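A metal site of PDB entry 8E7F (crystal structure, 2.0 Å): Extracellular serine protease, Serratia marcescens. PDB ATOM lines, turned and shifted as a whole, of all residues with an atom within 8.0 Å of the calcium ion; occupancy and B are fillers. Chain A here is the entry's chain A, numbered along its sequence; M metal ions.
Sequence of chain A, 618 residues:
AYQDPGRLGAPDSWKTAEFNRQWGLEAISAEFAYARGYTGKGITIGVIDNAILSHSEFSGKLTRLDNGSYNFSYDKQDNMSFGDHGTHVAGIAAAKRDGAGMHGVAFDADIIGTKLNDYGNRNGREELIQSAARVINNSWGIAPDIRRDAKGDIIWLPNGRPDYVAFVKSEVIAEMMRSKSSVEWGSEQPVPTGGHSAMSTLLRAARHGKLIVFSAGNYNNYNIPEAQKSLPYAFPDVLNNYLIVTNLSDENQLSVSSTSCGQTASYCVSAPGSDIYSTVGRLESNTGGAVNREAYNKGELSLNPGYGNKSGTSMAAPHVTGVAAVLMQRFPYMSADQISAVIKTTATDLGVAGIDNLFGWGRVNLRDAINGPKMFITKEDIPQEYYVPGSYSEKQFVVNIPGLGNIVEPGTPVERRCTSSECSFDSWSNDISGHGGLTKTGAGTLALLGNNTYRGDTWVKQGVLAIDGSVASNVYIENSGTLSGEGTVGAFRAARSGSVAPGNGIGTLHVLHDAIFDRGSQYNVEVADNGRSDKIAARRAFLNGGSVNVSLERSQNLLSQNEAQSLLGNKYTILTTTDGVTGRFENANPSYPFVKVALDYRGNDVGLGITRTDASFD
The side-chain carboxylate of Glu 18 sits at hydrogen-bond distance from the backbone NH of Gly 99 (2.9 Å).
The side-chain carboxylate (OE1) of Glu 57 sits close to the side-chain hydroxyl (OH) of Tyr 307, 2.6 Å away.
Six residues have an atom within 4 Å of the calcium ion: Glu 18, Glu 57, Lys 96, Asp 98, Ala 100 and Met 102.
The calcium ion is bound by the backbone carbonyl oxygen (O) of Ala 100 (2.3 Å), the side-chain carboxylate (OE2) of Glu 18 (2.3 Å), the side-chain carboxylate (OE2) of Glu 57 (2.3 Å), the backbone carbonyl oxygen (O) of Met 102 (2.4 Å), the side-chain carboxylate (OE1) of Glu 57 (2.4 Å), the backbone carbonyl oxygen (O) of Lys 96 (2.4 Å) and the side-chain carboxylate (OD1) of Asp 98 (2.6 Å).
The calcium ion has seven donor atoms within binding distance.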
ATOM      1  N   TYR A   2      -0.888  -8.924 -13.804  1.00  0.00           N
ATOM      2  CA  TYR A   2      -0.231  -8.109 -14.866  1.00  0.00           C
ATOM      3  C   TYR A   2      -1.209  -7.937 -16.029  1.00  0.00           C
ATOM      4  O   TYR A   2      -1.628  -8.971 -16.570  1.00  0.00           O
ATOM      5  CB  TYR A   2       1.041  -8.786 -15.395  1.00  0.00           C
ATOM      6  CG  TYR A   2       1.744  -8.020 -16.486  1.00  0.00           C
ATOM      7  CD1 TYR A   2       2.063  -6.684 -16.296  1.00  0.00           C
ATOM      8  CD2 TYR A   2       2.075  -8.602 -17.702  1.00  0.00           C
ATOM      9  CE1 TYR A   2       2.686  -5.935 -17.285  1.00  0.00           C
ATOM     10  CE2 TYR A   2       2.721  -7.872 -18.696  1.00  0.00           C
ATOM     11  CZ  TYR A   2       3.031  -6.532 -18.478  1.00  0.00           C
ATOM     12  OH  TYR A   2       3.678  -5.765 -19.399  1.00  0.00           O
ATOM     13  N   GLU A  18       9.881  -4.178 -19.259  1.00  0.00           N
ATOM     14  CA  GLU A  18      10.301  -5.594 -19.186  1.00  0.00           C
ATOM     15  C   GLU A  18      11.029  -5.974 -20.481  1.00  0.00           C
ATOM     16  O   GLU A  18      12.148  -6.485 -20.384  1.00  0.00           O
ATOM     17  CB  GLU A  18       9.108  -6.509 -18.948  1.00  0.00           C
ATOM     18  CG  GLU A  18       9.467  -7.986 -18.866  1.00  0.00           C
ATOM     19  CD  GLU A  18       8.264  -8.849 -18.543  1.00  0.00           C
ATOM     20  OE1 GLU A  18       7.152  -8.399 -18.888  1.00  0.00           O
ATOM     21  OE2 GLU A  18       8.436  -9.955 -17.947  1.00  0.00           O
ATOM     22  N   PHE A  19      10.415  -5.712 -21.632  1.00  0.00           N
ATOM     23  CA  PHE A  19      10.921  -6.020 -22.994  1.00  0.00           C
ATOM     24  C   PHE A  19      12.276  -5.335 -23.210  1.00  0.00           C
ATOM     25  O   PHE A  19      13.220  -5.978 -23.712  1.00  0.00           O
ATOM     26  CB  PHE A  19       9.934  -5.536 -24.046  1.00  0.00           C
ATOM     27  CG  PHE A  19      10.365  -5.723 -25.471  1.00  0.00           C
ATOM     28  CD1 PHE A  19      11.105  -4.757 -26.120  1.00  0.00           C
ATOM     29  CD2 PHE A  19      10.010  -6.872 -26.172  1.00  0.00           C
ATOM     30  CE1 PHE A  19      11.480  -4.921 -27.445  1.00  0.00           C
ATOM     31  CE2 PHE A  19      10.394  -7.026 -27.493  1.00  0.00           C
ATOM     32  CZ  PHE A  19      11.136  -6.053 -28.114  1.00  0.00           C
ATOM     33  N   ARG A  21      14.503  -4.237 -21.124  1.00  0.00           N
ATOM     34  CA  ARG A  21      15.628  -4.652 -20.224  1.00  0.00           C
ATOM     35  C   ARG A  21      16.530  -5.693 -20.897  1.00  0.00           C
ATOM     36  O   ARG A  21      17.660  -5.850 -20.374  1.00  0.00           O
ATOM     37  CB  ARG A  21      15.091  -5.172 -18.882  1.00  0.00           C
ATOM     38  CG  ARG A  21      14.754  -4.060 -17.909  1.00  0.00           C
ATOM     39  CD  ARG A  21      14.142  -4.513 -16.605  1.00  0.00           C
ATOM     40  NE  ARG A  21      13.274  -3.482 -16.018  1.00  0.00           N
ATOM     41  CZ  ARG A  21      11.972  -3.620 -15.706  1.00  0.00           C
ATOM     42  NH1 ARG A  21      11.340  -4.768 -15.879  1.00  0.00           N
ATOM     43  NH2 ARG A  21      11.301  -2.593 -15.210  1.00  0.00           N
ATOM     44  N   HIS A  55      12.500 -20.455 -10.424  1.00  0.00           N
ATOM     45  CA  HIS A  55      12.541 -18.981 -10.477  1.00  0.00           C
ATOM     46  C   HIS A  55      11.102 -18.640 -10.817  1.00  0.00           C
ATOM     47  O   HIS A  55      10.497 -19.449 -11.537  1.00  0.00           O
ATOM     48  CB  HIS A  55      13.601 -18.493 -11.482  1.00  0.00           C
ATOM     49  CG  HIS A  55      13.882 -17.034 -11.496  1.00  0.00           C
ATOM     50  ND1 HIS A  55      15.166 -16.547 -11.379  1.00  0.00           N
ATOM     51  CD2 HIS A  55      13.075 -15.961 -11.622  1.00  0.00           C
ATOM     52  CE1 HIS A  55      15.142 -15.236 -11.418  1.00  0.00           C
ATOM     53  NE2 HIS A  55      13.864 -14.845 -11.574  1.00  0.00           N
ATOM     54  N   SER A  56      10.564 -17.547 -10.291  1.00  0.00           N
ATOM     55  CA  SER A  56       9.256 -16.962 -10.666  1.00  0.00           C
ATOM     56  C   SER A  56       9.093 -16.929 -12.181  1.00  0.00           C
ATOM     57  O   SER A  56       7.965 -17.137 -12.666  1.00  0.00           O
ATOM     58  CB  SER A  56       9.139 -15.562 -10.118  1.00  0.00           C
ATOM     59  OG  SER A  56       9.120 -15.603  -8.707  1.00  0.00           O
ATOM     60  N   GLU A  57      10.171 -16.641 -12.908  1.00  0.00           N
ATOM     61  CA  GLU A  57      10.131 -16.395 -14.378  1.00  0.00           C
ATOM     62  C   GLU A  57       9.755 -17.684 -15.108  1.00  0.00           C
ATOM     63  O   GLU A  57       9.339 -17.576 -16.255  1.00  0.00           O
ATOM     64  CB  GLU A  57      11.458 -15.838 -14.892  1.00  0.00           C
ATOM     65  CG  GLU A  57      11.702 -14.378 -14.521  1.00  0.00           C
ATOM     66  CD  GLU A  57      10.813 -13.340 -15.177  1.00  0.00           C
ATOM     67  OE1 GLU A  57      10.918 -12.156 -14.815  1.00  0.00           O
ATOM     68  OE2 GLU A  57      10.019 -13.703 -16.062  1.00  0.00           O
ATOM     69  N   PHE A  58       9.888 -18.833 -14.473  1.00  0.00           N
ATOM     70  CA  PHE A  58       9.552 -20.159 -15.053  1.00  0.00           C
ATOM     71  C   PHE A  58       8.397 -20.840 -14.315  1.00  0.00           C
ATOM     72  O   PHE A  58       8.157 -22.027 -14.604  1.00  0.00           O
ATOM     73  CB  PHE A  58      10.773 -21.080 -15.017  1.00  0.00           C
ATOM     74  CG  PHE A  58      12.049 -20.431 -15.496  1.00  0.00           C
ATOM     75  CD1 PHE A  58      12.094 -19.764 -16.717  1.00  0.00           C
ATOM     76  CD2 PHE A  58      13.193 -20.482 -14.735  1.00  0.00           C
ATOM     77  CE1 PHE A  58      13.258 -19.156 -17.152  1.00  0.00           C
ATOM     78  CE2 PHE A  58      14.366 -19.863 -15.166  1.00  0.00           C
ATOM     79  CZ  PHE A  58      14.383 -19.199 -16.370  1.00  0.00           C
ATOM     80  N   GLY A  91      16.261 -18.329 -19.362  1.00  0.00           N
ATOM     81  CA  GLY A  91      15.571 -17.028 -19.252  1.00  0.00           C
ATOM     82  C   GLY A  91      15.537 -16.309 -20.580  1.00  0.00           C
ATOM     83  O   GLY A  91      14.456 -15.729 -20.931  1.00  0.00           O
ATOM     84  N   ALA A  94      12.922 -18.231 -22.708  1.00  0.00           N
ATOM     85  CA  ALA A  94      11.512 -18.474 -22.311  1.00  0.00           C
ATOM     86  C   ALA A  94      11.124 -17.942 -20.922  1.00  0.00           C
ATOM     87  O   ALA A  94      10.099 -18.377 -20.436  1.00  0.00           O
ATOM     88  CB  ALA A  94      11.262 -19.946 -22.433  1.00  0.00           C
ATOM     89  N   ALA A  95      11.811 -16.961 -20.335  1.00  0.00           N
ATOM     90  CA  ALA A  95      11.304 -16.247 -19.142  1.00  0.00           C
ATOM     91  C   ALA A  95       9.893 -15.679 -19.436  1.00  0.00           C
ATOM     92  O   ALA A  95       9.668 -15.156 -20.540  1.00  0.00           O
ATOM     93  CB  ALA A  95      12.255 -15.159 -18.708  1.00  0.00           C
ATOM     94  N   LYS A  96       9.022 -15.713 -18.447  1.00  0.00           N
ATOM     95  CA  LYS A  96       7.631 -15.201 -18.513  1.00  0.00           C
ATOM     96  C   LYS A  96       7.616 -13.722 -18.832  1.00  0.00           C
ATOM     97  O   LYS A  96       8.389 -12.968 -18.255  1.00  0.00           O
ATOM     98  CB  LYS A  96       6.855 -15.396 -17.201  1.00  0.00           C
ATOM     99  CG  LYS A  96       6.214 -16.779 -17.102  1.00  0.00           C
ATOM    100  CD  LYS A  96       5.784 -17.176 -15.712  1.00  0.00           C
ATOM    101  CE  LYS A  96       4.598 -16.367 -15.221  1.00  0.00           C
ATOM    102  NZ  LYS A  96       3.384 -17.200 -15.070  1.00  0.00           N
ATOM    103  N   ARG A  97       6.703 -13.332 -19.682  1.00  0.00           N
ATOM    104  CA  ARG A  97       6.353 -11.908 -19.862  1.00  0.00           C
ATOM    105  C   ARG A  97       5.253 -11.639 -18.834  1.00  0.00           C
ATOM    106  O   ARG A  97       4.114 -11.986 -19.117  1.00  0.00           O
ATOM    107  CB  ARG A  97       5.926 -11.647 -21.306  1.00  0.00           C
ATOM    108  CG  ARG A  97       5.652 -10.188 -21.598  1.00  0.00           C
ATOM    109  CD  ARG A  97       5.268 -10.009 -23.057  1.00  0.00           C
ATOM    110  NE  ARG A  97       4.666  -8.697 -23.200  1.00  0.00           N
ATOM    111  CZ  ARG A  97       5.238  -7.594 -23.665  1.00  0.00           C
ATOM    112  NH1 ARG A  97       6.486  -7.570 -24.102  1.00  0.00           N
ATOM    113  NH2 ARG A  97       4.536  -6.482 -23.689  1.00  0.00           N
ATOM    114  N   ASP A  98       5.637 -11.155 -17.653  1.00  0.00           N
ATOM    115  CA  ASP A  98       4.739 -11.046 -16.468  1.00  0.00           C
ATOM    116  C   ASP A  98       4.871  -9.640 -15.855  1.00  0.00           C
ATOM    117  O   ASP A  98       4.429  -9.471 -14.708  1.00  0.00           O
ATOM    118  CB  ASP A  98       5.062 -12.154 -15.454  1.00  0.00           C
ATOM    119  CG  ASP A  98       6.496 -12.121 -14.950  1.00  0.00           C
ATOM    120  OD1 ASP A  98       7.228 -11.217 -15.348  1.00  0.00           O
ATOM    121  OD2 ASP A  98       6.852 -13.005 -14.171  1.00  0.00           O
ATOM    122  N   GLY A  99       5.434  -8.693 -16.591  1.00  0.00           N
ATOM    123  CA  GLY A  99       5.693  -7.324 -16.102  1.00  0.00           C
ATOM    124  C   GLY A  99       6.830  -7.258 -15.104  1.00  0.00           C
ATOM    125  O   GLY A  99       7.026  -6.188 -14.507  1.00  0.00           O
ATOM    126  N   ALA A 100       7.593  -8.331 -14.895  1.00  0.00           N
ATOM    127  CA  ALA A 100       8.706  -8.319 -13.929  1.00  0.00           C
ATOM    128  C   ALA A 100      10.021  -8.718 -14.610  1.00  0.00           C
ATOM    129  O   ALA A 100       9.998  -9.662 -15.438  1.00  0.00           O
ATOM    130  CB  ALA A 100       8.375  -9.200 -12.757  1.00  0.00           C
ATOM    131  N   GLY A 101      11.115  -8.005 -14.282  1.00  0.00           N
ATOM    132  CA  GLY A 101      12.498  -8.252 -14.731  1.00  0.00           C
ATOM    133  C   GLY A 101      12.616  -8.199 -16.251  1.00  0.00           C
ATOM    134  O   GLY A 101      12.468  -7.099 -16.818  1.00  0.00           O
ATOM    135  N   MET A 102      12.827  -9.352 -16.898  1.00  0.00           N
ATOM    136  CA  MET A 102      12.902  -9.445 -18.372  1.00  0.00           C
ATOM    137  C   MET A 102      12.046 -10.629 -18.828  1.00  0.00           C
ATOM    138  O   MET A 102      11.478 -11.292 -17.976  1.00  0.00           O
ATOM    139  CB  MET A 102      14.365  -9.582 -18.862  1.00  0.00           C
ATOM    140  CG  MET A 102      15.228 -10.503 -18.062  1.00  0.00           C
ATOM    141  SD  MET A 102      14.760 -12.239 -18.256  1.00  0.00           S
ATOM    142  CE  MET A 102      15.286 -12.479 -19.964  1.00  0.00           C
ATOM    143  N   HIS A 103      11.951 -10.886 -20.122  1.00  0.00           N
ATOM    144  CA  HIS A 103      11.215 -12.078 -20.620  1.00  0.00           C
ATOM    145  C   HIS A 103      11.941 -12.693 -21.802  1.00  0.00           C
ATOM    146  O   HIS A 103      12.815 -12.031 -22.412  1.00  0.00           O
ATOM    147  CB  HIS A 103       9.760 -11.737 -20.908  1.00  0.00           C
ATOM    148  CG  HIS A 103       9.533 -10.862 -22.083  1.00  0.00           C
ATOM    149  ND1 HIS A 103       9.809 -11.278 -23.373  1.00  0.00           N
ATOM    150  CD2 HIS A 103       8.968  -9.640 -22.196  1.00  0.00           C
ATOM    151  CE1 HIS A 103       9.448 -10.333 -24.208  1.00  0.00           C
ATOM    152  NE2 HIS A 103       8.938  -9.313 -23.517  1.00  0.00           N
ATOM    153  N   GLY A 104      11.577 -13.931 -22.088  1.00  0.00           N
ATOM    154  CA  GLY A 104      12.234 -14.735 -23.127  1.00  0.00           C
ATOM    155  C   GLY A 104      11.768 -14.313 -24.493  1.00  0.00           C
ATOM    156  O   GLY A 104      10.743 -13.575 -24.604  1.00  0.00           O
ATOM    157  N   PHE A 107       8.232 -16.245 -24.890  1.00  0.00           N
ATOM    158  CA  PHE A 107       7.814 -16.022 -23.481  1.00  0.00           C
ATOM    159  C   PHE A 107       6.619 -16.910 -23.103  1.00  0.00           C
ATOM    160  O   PHE A 107       6.416 -17.052 -21.892  1.00  0.00           O
ATOM    161  CB  PHE A 107       7.575 -14.532 -23.225  1.00  0.00           C
ATOM    162  CG  PHE A 107       6.480 -13.882 -24.037  1.00  0.00           C
ATOM    163  CD1 PHE A 107       5.152 -14.114 -23.733  1.00  0.00           C
ATOM    164  CD2 PHE A 107       6.792 -12.970 -25.026  1.00  0.00           C
ATOM    165  CE1 PHE A 107       4.150 -13.482 -24.453  1.00  0.00           C
ATOM    166  CE2 PHE A 107       5.792 -12.354 -25.758  1.00  0.00           C
ATOM    167  CZ  PHE A 107       4.467 -12.608 -25.457  1.00  0.00           C
ATOM    168  N   THR A 279      17.737 -14.318 -16.173  1.00  0.00           N
ATOM    169  CA  THR A 279      17.535 -14.975 -14.866  1.00  0.00           C
ATOM    170  C   THR A 279      18.834 -15.619 -14.370  1.00  0.00           C
ATOM    171  O   THR A 279      19.501 -16.345 -15.165  1.00  0.00           O
ATOM    172  CB  THR A 279      16.398 -15.989 -14.972  1.00  0.00           C
ATOM    173  OG1 THR A 279      16.655 -16.772 -16.137  1.00  0.00           O
ATOM    174  CG2 THR A 279      15.049 -15.304 -15.054  1.00  0.00           C
ATOM    175  N   TYR A 307      18.526 -11.600 -11.225  1.00  0.00           N
ATOM    176  CA  TYR A 307      18.899 -11.286 -12.610  1.00  0.00           C
ATOM    177  C   TYR A 307      20.335 -10.804 -12.623  1.00  0.00           C
ATOM    178  O   TYR A 307      20.828 -10.320 -11.586  1.00  0.00           O
ATOM    179  CB  TYR A 307      17.964 -10.234 -13.187  1.00  0.00           C
ATOM    180  CG  TYR A 307      16.510 -10.614 -13.077  1.00  0.00           C
ATOM    181  CD1 TYR A 307      15.915 -11.385 -14.065  1.00  0.00           C
ATOM    182  CD2 TYR A 307      15.753 -10.234 -11.983  1.00  0.00           C
ATOM    183  CE1 TYR A 307      14.586 -11.740 -13.990  1.00  0.00           C
ATOM    184  CE2 TYR A 307      14.418 -10.602 -11.890  1.00  0.00           C
ATOM    185  CZ  TYR A 307      13.827 -11.347 -12.898  1.00  0.00           C
ATOM    186  OH  TYR A 307      12.516 -11.697 -12.846  1.00  0.00           O
HETATM  187 CA    CA M   1       9.497 -11.514 -16.661  1.00  0.00          CA
